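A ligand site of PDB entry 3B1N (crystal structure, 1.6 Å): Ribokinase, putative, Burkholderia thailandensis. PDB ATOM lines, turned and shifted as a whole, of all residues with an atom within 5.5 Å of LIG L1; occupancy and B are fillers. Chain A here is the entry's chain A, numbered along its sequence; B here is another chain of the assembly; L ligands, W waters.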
ATOM      1  N   SER A   8     -19.094   3.104  -9.811  1.00  0.00           N
ATOM      2  CA  SER A   8     -18.618   3.289 -11.180  1.00  0.00           C
ATOM      3  C   SER A   8     -17.109   3.121 -11.363  1.00  0.00           C
ATOM      4  O   SER A   8     -16.316   3.456 -10.461  1.00  0.00           O
ATOM      5  CB  SER A   8     -19.027   4.669 -11.688  1.00  0.00           C
ATOM      6  OG  SER A   8     -18.455   5.695 -10.898  1.00  0.00           O
ATOM      7  N   ALA A  10     -14.603   4.287 -14.443  1.00  0.00           N
ATOM      8  CA  ALA A  10     -14.829   5.211 -15.589  1.00  0.00           C
ATOM      9  C   ALA A  10     -13.570   5.890 -16.017  1.00  0.00           C
ATOM     10  O   ALA A  10     -12.635   6.021 -15.253  1.00  0.00           O
ATOM     11  CB  ALA A  10     -15.940   6.259 -15.221  1.00  0.00           C
ATOM     12  N   TYR A  11     -13.583   6.416 -17.257  1.00  0.00           N
ATOM     13  CA  TYR A  11     -12.527   7.333 -17.671  1.00  0.00           C
ATOM     14  C   TYR A  11     -13.031   8.742 -17.616  1.00  0.00           C
ATOM     15  O   TYR A  11     -14.151   9.005 -18.056  1.00  0.00           O
ATOM     16  CB  TYR A  11     -12.121   7.009 -19.118  1.00  0.00           C
ATOM     17  CG  TYR A  11     -11.496   5.659 -19.258  1.00  0.00           C
ATOM     18  CD1 TYR A  11     -10.251   5.413 -18.699  1.00  0.00           C
ATOM     19  CD2 TYR A  11     -12.128   4.631 -19.931  1.00  0.00           C
ATOM     20  CE1 TYR A  11      -9.638   4.165 -18.849  1.00  0.00           C
ATOM     21  CE2 TYR A  11     -11.528   3.363 -20.086  1.00  0.00           C
ATOM     22  CZ  TYR A  11     -10.275   3.155 -19.550  1.00  0.00           C
ATOM     23  OH  TYR A  11      -9.685   1.884 -19.683  1.00  0.00           O
ATOM     24  N   ASP A  12     -12.244   9.629 -17.030  1.00  0.00           N
ATOM     25  CA  ASP A  12     -12.677  10.983 -16.794  1.00  0.00           C
ATOM     26  C   ASP A  12     -11.960  11.961 -17.695  1.00  0.00           C
ATOM     27  O   ASP A  12     -10.756  11.879 -17.837  1.00  0.00           O
ATOM     28  CB  ASP A  12     -12.383  11.445 -15.360  1.00  0.00           C
ATOM     29  CG  ASP A  12     -13.210  10.697 -14.303  1.00  0.00           C
ATOM     30  OD1 ASP A  12     -14.246  10.099 -14.627  1.00  0.00           O
ATOM     31  OD2 ASP A  12     -12.761  10.828 -13.117  1.00  0.00           O
ATOM     32  N   GLY A  47     -10.713   7.007 -13.454  1.00  0.00           N
ATOM     33  CA  GLY A  47     -11.679   7.558 -12.522  1.00  0.00           C
ATOM     34  C   GLY A  47     -12.788   6.566 -12.228  1.00  0.00           C
ATOM     35  O   GLY A  47     -12.584   5.317 -12.208  1.00  0.00           O
ATOM     36  N   GLY A  48     -13.993   7.107 -11.999  1.00  0.00           N
ATOM     37  CA  GLY A  48     -15.095   6.308 -11.450  1.00  0.00           C
ATOM     38  C   GLY A  48     -15.015   6.261  -9.920  1.00  0.00           C
ATOM     39  O   GLY A  48     -13.909   6.234  -9.378  1.00  0.00           O
ATOM     40  N   CYS A  49     -16.155   6.281  -9.248  1.00  0.00           N
ATOM     41  CA  CYS A  49     -16.155   6.331  -7.789  1.00  0.00           C
ATOM     42  C   CYS A  49     -15.554   5.090  -7.231  1.00  0.00           C
ATOM     43  O   CYS A  49     -14.738   5.206  -6.293  1.00  0.00           O
ATOM     44  CB  CYS A  49     -17.586   6.523  -7.285  1.00  0.00           C
ATOM     45  SG  CYS A  49     -18.313   8.099  -7.966  1.00  0.00           S
ATOM     46  N   ASN A  52     -11.718   5.330  -7.736  1.00  0.00           N
ATOM     47  CA  ASN A  52     -11.126   6.335  -6.895  1.00  0.00           C
ATOM     48  C   ASN A  52     -11.069   5.886  -5.447  1.00  0.00           C
ATOM     49  O   ASN A  52     -10.022   6.060  -4.807  1.00  0.00           O
ATOM     50  CB  ASN A  52     -11.886   7.664  -6.993  1.00  0.00           C
ATOM     51  CG  ASN A  52     -11.896   8.261  -8.380  1.00  0.00           C
ATOM     52  OD1 ASN A  52     -11.050   7.961  -9.254  1.00  0.00           O
ATOM     53  ND2 ASN A  52     -12.823   9.180  -8.592  1.00  0.00           N
ATOM     54  N   ALA A 103     -16.847  10.115 -18.055  1.00  0.00           N
ATOM     55  CA  ALA A 103     -17.365  11.337 -17.436  1.00  0.00           C
ATOM     56  C   ALA A 103     -16.710  12.571 -18.014  1.00  0.00           C
ATOM     57  O   ALA A 103     -15.500  12.661 -18.066  1.00  0.00           O
ATOM     58  CB  ALA A 103     -17.077  11.331 -15.921  1.00  0.00           C
ATOM     59  N   ILE A 105     -16.281  16.234 -17.009  1.00  0.00           N
ATOM     60  CA  ILE A 105     -16.531  16.943 -15.775  1.00  0.00           C
ATOM     61  C   ILE A 105     -16.011  18.369 -15.882  1.00  0.00           C
ATOM     62  O   ILE A 105     -14.810  18.565 -16.120  1.00  0.00           O
ATOM     63  CB  ILE A 105     -15.752  16.257 -14.624  1.00  0.00           C
ATOM     64  CG1 ILE A 105     -16.245  14.821 -14.451  1.00  0.00           C
ATOM     65  CG2 ILE A 105     -15.930  17.042 -13.337  1.00  0.00           C
ATOM     66  CD1 ILE A 105     -15.481  14.028 -13.399  1.00  0.00           C
ATOM     67  N   GLN A 113     -18.833  20.382  -9.436  1.00  0.00           N
ATOM     68  CA  GLN A 113     -18.763  19.490 -10.562  1.00  0.00           C
ATOM     69  C   GLN A 113     -20.065  19.479 -11.309  1.00  0.00           C
ATOM     70  O   GLN A 113     -21.102  19.083 -10.744  1.00  0.00           O
ATOM     71  CB  GLN A 113     -18.425  18.005 -10.210  1.00  0.00           C
ATOM     72  CG  GLN A 113     -17.030  17.854  -9.640  1.00  0.00           C
ATOM     73  CD  GLN A 113     -16.703  16.432  -9.280  1.00  0.00           C
ATOM     74  OE1 GLN A 113     -17.080  15.496  -9.980  1.00  0.00           O
ATOM     75  NE2 GLN A 113     -15.994  16.255  -8.177  1.00  0.00           N
ATOM     76  N   THR A 115     -21.293  17.560 -14.436  1.00  0.00           N
ATOM     77  CA  THR A 115     -20.805  16.409 -15.200  1.00  0.00           C
ATOM     78  C   THR A 115     -21.800  15.879 -16.214  1.00  0.00           C
ATOM     79  O   THR A 115     -22.977  15.629 -15.899  1.00  0.00           O
ATOM     80  CB  THR A 115     -20.419  15.268 -14.263  1.00  0.00           C
ATOM     81  OG1 THR A 115     -19.350  15.755 -13.407  1.00  0.00           O
ATOM     82  CG2 THR A 115     -19.947  14.038 -15.022  1.00  0.00           C
ATOM     83  N   PHE A 117     -22.364  12.588 -18.163  1.00  0.00           N
ATOM     84  CA  PHE A 117     -21.917  11.223 -17.971  1.00  0.00           C
ATOM     85  C   PHE A 117     -22.377  10.306 -19.098  1.00  0.00           C
ATOM     86  O   PHE A 117     -23.590  10.284 -19.429  1.00  0.00           O
ATOM     87  CB  PHE A 117     -22.434  10.714 -16.628  1.00  0.00           C
ATOM     88  CG  PHE A 117     -21.657   9.543 -16.079  1.00  0.00           C
ATOM     89  CD1 PHE A 117     -20.402   9.759 -15.512  1.00  0.00           C
ATOM     90  CD2 PHE A 117     -22.167   8.251 -16.121  1.00  0.00           C
ATOM     91  CE1 PHE A 117     -19.661   8.703 -15.015  1.00  0.00           C
ATOM     92  CE2 PHE A 117     -21.408   7.172 -15.614  1.00  0.00           C
ATOM     93  CZ  PHE A 117     -20.175   7.405 -15.064  1.00  0.00           C
ATOM     94  N   MET A 122     -21.596   0.860 -17.370  1.00  0.00           N
ATOM     95  CA  MET A 122     -22.137   1.109 -16.029  1.00  0.00           C
ATOM     96  C   MET A 122     -23.634   0.766 -16.021  1.00  0.00           C
ATOM     97  O   MET A 122     -24.195   0.370 -14.965  1.00  0.00           O
ATOM     98  CB  MET A 122     -21.915   2.546 -15.566  1.00  0.00           C
ATOM     99  CG  MET A 122     -22.281   2.732 -14.105  1.00  0.00           C
ATOM    100  SD  MET A 122     -22.227   4.412 -13.566  1.00  0.00           S
ATOM    101  CE  MET A 122     -23.835   5.068 -14.092  1.00  0.00           C
ATOM    102  N   PRO A 143     -22.021   5.746  -6.432  1.00  0.00           N
ATOM    103  CA  PRO A 143     -22.773   6.014  -7.662  1.00  0.00           C
ATOM    104  C   PRO A 143     -22.524   4.941  -8.696  1.00  0.00           C
ATOM    105  O   PRO A 143     -21.372   4.544  -8.921  1.00  0.00           O
ATOM    106  CB  PRO A 143     -22.135   7.383  -8.135  1.00  0.00           C
ATOM    107  CG  PRO A 143     -21.772   8.010  -6.865  1.00  0.00           C
ATOM    108  CD  PRO A 143     -21.171   6.894  -6.032  1.00  0.00           C
ATOM    109  N   ASP A 144     -23.567   4.515  -9.377  1.00  0.00           N
ATOM    110  CA  ASP A 144     -23.512   3.346 -10.255  1.00  0.00           C
ATOM    111  C   ASP A 144     -24.814   3.333 -11.044  1.00  0.00           C
ATOM    112  O   ASP A 144     -25.619   4.215 -10.904  1.00  0.00           O
ATOM    113  CB  ASP A 144     -23.482   2.098  -9.367  1.00  0.00           C
ATOM    114  CG  ASP A 144     -22.600   0.999  -9.898  1.00  0.00           C
ATOM    115  OD1 ASP A 144     -22.408   0.898 -11.130  1.00  0.00           O
ATOM    116  OD2 ASP A 144     -22.043   0.230  -9.086  1.00  0.00           O
ATOM    117  N   GLN A 169     -23.516  11.261  -7.087  1.00  0.00           N
ATOM    118  CA  GLN A 169     -24.029  11.661  -8.427  1.00  0.00           C
ATOM    119  C   GLN A 169     -25.231  10.857  -8.884  1.00  0.00           C
ATOM    120  O   GLN A 169     -25.918  11.263  -9.842  1.00  0.00           O
ATOM    121  CB  GLN A 169     -22.904  11.557  -9.458  1.00  0.00           C
ATOM    122  CG  GLN A 169     -21.803  12.584  -9.197  1.00  0.00           C
ATOM    123  CD  GLN A 169     -20.601  12.015  -8.423  1.00  0.00           C
ATOM    124  OE1 GLN A 169     -20.733  11.138  -7.557  1.00  0.00           O
ATOM    125  NE2 GLN A 169     -19.395  12.515  -8.740  1.00  0.00           N
ATOM    126  N   GLY A 170     -25.432   9.688  -8.270  1.00  0.00           N
ATOM    127  CA  GLY A 170     -26.596   8.855  -8.581  1.00  0.00           C
ATOM    128  C   GLY A 170     -27.872   9.287  -7.882  1.00  0.00           C
ATOM    129  O   GLY A 170     -28.895   8.684  -8.123  1.00  0.00           O
ATOM    130  N   THR A 249     -11.472  17.300  -7.959  1.00  0.00           N
ATOM    131  CA  THR A 249     -12.270  16.181  -8.468  1.00  0.00           C
ATOM    132  C   THR A 249     -11.755  14.867  -7.887  1.00  0.00           C
ATOM    133  O   THR A 249     -10.570  14.538  -8.048  1.00  0.00           O
ATOM    134  CB  THR A 249     -12.123  16.097 -10.017  1.00  0.00           C
ATOM    135  OG1 THR A 249     -12.417  17.380 -10.557  1.00  0.00           O
ATOM    136  CG2 THR A 249     -13.118  15.047 -10.582  1.00  0.00           C
ATOM    137  N   GLY A 250     -12.599  14.180  -7.157  1.00  0.00           N
ATOM    138  CA  GLY A 250     -12.155  12.941  -6.491  1.00  0.00           C
ATOM    139  C   GLY A 250     -11.850  13.151  -5.044  1.00  0.00           C
ATOM    140  O   GLY A 250     -11.502  12.160  -4.400  1.00  0.00           O
ATOM    141  N   ASP A 253     -13.918  10.927  -2.826  1.00  0.00           N
ATOM    142  CA  ASP A 253     -13.612   9.518  -2.905  1.00  0.00           C
ATOM    143  C   ASP A 253     -12.314   9.197  -2.181  1.00  0.00           C
ATOM    144  O   ASP A 253     -12.191   8.137  -1.574  1.00  0.00           O
ATOM    145  CB  ASP A 253     -13.517   9.094  -4.361  1.00  0.00           C
ATOM    146  CG  ASP A 253     -14.869   9.028  -5.022  1.00  0.00           C
ATOM    147  OD1 ASP A 253     -15.862   8.788  -4.301  1.00  0.00           O
ATOM    148  OD2 ASP A 253     -14.922   9.193  -6.227  1.00  0.00           O
ATOM    149  N   PRO A 289      -8.205  12.443 -10.473  1.00  0.00           N
ATOM    150  CA  PRO A 289      -8.650  11.874  -9.173  1.00  0.00           C
ATOM    151  C   PRO A 289      -7.652  10.942  -8.534  1.00  0.00           C
ATOM    152  O   PRO A 289      -7.699  10.764  -7.322  1.00  0.00           O
ATOM    153  CB  PRO A 289      -9.959  11.114  -9.528  1.00  0.00           C
ATOM    154  CG  PRO A 289     -10.053  11.099 -10.968  1.00  0.00           C
ATOM    155  CD  PRO A 289      -9.127  12.124 -11.579  1.00  0.00           C
ATOM    156  N   SER B  36     -24.976  15.920 -12.338  1.00  0.00           N
ATOM    157  CA  SER B  36     -24.424  14.845 -13.144  1.00  0.00           C
ATOM    158  C   SER B  36     -25.608  14.321 -13.922  1.00  0.00           C
ATOM    159  O   SER B  36     -26.591  13.824 -13.355  1.00  0.00           O
ATOM    160  CB  SER B  36     -23.740  13.757 -12.264  1.00  0.00           C
ATOM    161  OG  SER B  36     -23.102  12.769 -13.090  1.00  0.00           O
HETATM  162  N1  LIG L   1     -22.571   8.003 -11.844  1.00  0.00           N
HETATM  163  O1  LIG L   1     -19.949   7.906 -11.219  1.00  0.00           O
HETATM  164  C1  LIG L   1     -20.008   9.250 -11.622  1.00  0.00           C
HETATM  165  C2  LIG L   1     -21.201   9.934 -12.104  1.00  0.00           C
HETATM  166  C3  LIG L   1     -22.506   9.266 -12.200  1.00  0.00           C
HETATM  167  O2  LIG L   1     -23.496   9.944 -12.610  1.00  0.00           O
HETATM  168  N2  LIG L   1     -20.776  11.190 -12.356  1.00  0.00           N
HETATM  169  C4  LIG L   1     -19.434  11.313 -12.092  1.00  0.00           C
HETATM  170  N3  LIG L   1     -18.950  10.080 -11.679  1.00  0.00           N
HETATM  171  C5  LIG L   1     -17.583   9.802 -11.212  1.00  0.00           C
HETATM  172  C6  LIG L   1     -16.452  10.250 -12.112  1.00  0.00           C
HETATM  173  O3  LIG L   1     -16.131   9.150 -12.961  1.00  0.00           O
HETATM  174  C7  LIG L   1     -15.387  10.746 -11.120  1.00  0.00           C
HETATM  175  O4  LIG L   1     -14.164   9.952 -11.184  1.00  0.00           O
HETATM  176  C8  LIG L   1     -16.021  10.641  -9.738  1.00  0.00           C
HETATM  177  O5  LIG L   1     -17.431  10.622 -10.069  1.00  0.00           O
HETATM  178  C9  LIG L   1     -15.760  11.879  -8.884  1.00  0.00           C
HETATM  179  O6  LIG L   1     -16.160  11.833  -7.447  1.00  0.00           O
HETATM  180  P1  LG2 L   2     -16.886  15.798  -2.816  1.00  0.00           P
HETATM  181  O1  LG2 L   2     -15.630  15.545  -3.674  1.00  0.00           O
HETATM  182  O2  LG2 L   2     -17.653  17.002  -3.243  1.00  0.00           O
HETATM  183  O3  LG2 L   2     -17.618  14.513  -2.621  1.00  0.00           O
HETATM  184  P2  LG2 L   2     -15.610  17.599  -0.831  1.00  0.00           P
HETATM  185  O4  LG2 L   2     -16.499  17.915   0.334  1.00  0.00           O
HETATM  186  O5  LG2 L   2     -15.329  18.690  -1.817  1.00  0.00           O
HETATM  187  O6  LG2 L   2     -16.147  16.268  -1.449  1.00  0.00           O
HETATM  188  O7  LG2 L   2     -14.134  17.175  -0.309  1.00  0.00           O
HETATM  189  C1  LG2 L   2     -13.982  15.990   0.518  1.00  0.00           C
HETATM  190  C2  LG2 L   2     -12.922  16.288   1.598  1.00  0.00           C
HETATM  191  O8  LG2 L   2     -11.669  16.602   0.920  1.00  0.00           O
HETATM  192  C3  LG2 L   2     -13.152  17.510   2.479  1.00  0.00           C
HETATM  193  O9  LG2 L   2     -14.061  17.142   3.535  1.00  0.00           O
HETATM  194  C4  LG2 L   2     -11.759  17.881   2.899  1.00  0.00           C
HETATM  195  O10 LG2 L   2     -11.355  17.015   3.959  1.00  0.00           O
HETATM  196  C5  LG2 L   2     -10.902  17.540   1.657  1.00  0.00           C
HETATM  197  N1  LG2 L   2     -10.845  18.796   0.902  1.00  0.00           N
HETATM  198  C6  LG2 L   2     -11.725  19.212  -0.050  1.00  0.00           C
HETATM  199  N2  LG2 L   2     -11.426  20.448  -0.545  1.00  0.00           N
HETATM  200  C7  LG2 L   2     -10.336  20.870   0.157  1.00  0.00           C
HETATM  201  C8  LG2 L   2      -9.509  22.070   0.200  1.00  0.00           C
HETATM  202  N3  LG2 L   2      -9.724  23.154  -0.565  1.00  0.00           N
HETATM  203  N4  LG2 L   2      -8.461  22.077   1.110  1.00  0.00           N
HETATM  204  C9  LG2 L   2      -8.178  20.995   1.852  1.00  0.00           C
HETATM  205  N5  LG2 L   2      -8.909  19.886   1.867  1.00  0.00           N
HETATM  206  C10 LG2 L   2      -9.981  19.787   1.047  1.00  0.00           C
HETATM  207  O   HOH W   1     -15.301  14.335  -6.218  1.00  0.00           O
HETATM  208  O   HOH W   2     -17.803  13.871  -6.734  1.00  0.00           O
HETATM  209  O   HOH W   3     -26.306   8.371 -13.118  1.00  0.00           O
HETATM  210  O   HOH W   4     -25.176   6.999 -11.304  1.00  0.00           O
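N of Ser 8 lies within hydrogen-bond range of O of Pro 143.
O of Gly 48 sits close to ND2 of Asn 52.
The side-chain carboxylate of Asp 253 lies within hydrogen-bond range of the side-chain amide nitrogen of Asn 52 (3.2 Å).
N of Cys 49 lies within hydrogen-bond range of OG of Ser 8 (2.9 Å).
The backbone NH of Ala 103 is in hydrogen-bond range of the backbone carbonyl oxygen of Tyr 11 (2.9 Å).
N of Gly 47 sits at hydrogen-bond distance from O of Ala 10 (2.8 Å).
Water W2 lies within hydrogen-bond range of an oxygen (O6) of LIG L1 (2.7 Å), the side-chain amide nitrogen (NE2) of Gln 169 (2.9 Å) and the side-chain amide nitrogen (NE2) of Gln 113 (3.3 Å).
Water W4 bridges a nitrogen (N1) of LIG L1 (2.8 Å) and the backbone carbonyl oxygen of Asp 144 (2.8 Å).
Water W1 lies within hydrogen-bond range of the side-chain amide nitrogen (NE2) of Gln 113 (2.8 Å), an oxygen (O1) of LG2 L2 (2.8 Å), the backbone NH (N) of Gly 250 (2.9 Å) and an oxygen (O6) of LIG L1 (2.9 Å).
Residues that only touch LIG L1: Phe 117 (3.5 Å), Ala 10 (3.7 Å), Gly 47 (3.7 Å), Pro 143 (3.8 Å), Ala 103 (3.8 Å), Met 122 (3.9 Å), Thr 115 (3.99 Å) and Ile 105 (3.997 Å).
Hydrophobic or aromatic side chains that line LIG L1: Ala 10, Ala 103, Ile 105, Phe 117, Met 122 and Pro 143.
16 residues have an atom within 4 Å of LIG L1: Ser 8, Ala 10, Asp 12, Gly 47, Gly 48, Cys 49, Asn 52, Ala 103, Ile 105, Thr 115, Phe 117, Met 122, Pro 143, Gln 169, Asp 253 and Ser 36 of chain B.
The nearest printed residue that does not touch LIG L1 is Gln 113 (4.003 Å).
The side-chain hydroxyl (OG) of Ser 8 lies within hydrogen-bond range of an oxygen (O1) of LIG L1.
The side-chain hydroxyl (OG) of Ser 36 of chain B lies within hydrogen-bond range of an oxygen (O2) of LIG L1, at 2.9 Å.
The side-chain carboxylate of Asp 12 sits at hydrogen-bond distance from an oxygen (O4) of LIG L1 (2.5 Å).
An oxygen (O5) of LIG L1 lies within hydrogen-bond range of the side-chain amide nitrogen of Gln 169.
N of Gly 48 is in hydrogen-bond range of O4 of LIG L1 (3.0 Å).
The side-chain amide nitrogen (ND2) of Asn 52 is in hydrogen-bond range of an oxygen (O4) of LIG L1, 3.0 Å away.
OD2 of Asp 253 lies within hydrogen-bond range of O6 of LIG L1, 3.2 Å away.
The side-chain sulfur of Cys 49 is in hydrogen-bond range of an oxygen (O5) of LIG L1 (3.4 Å).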
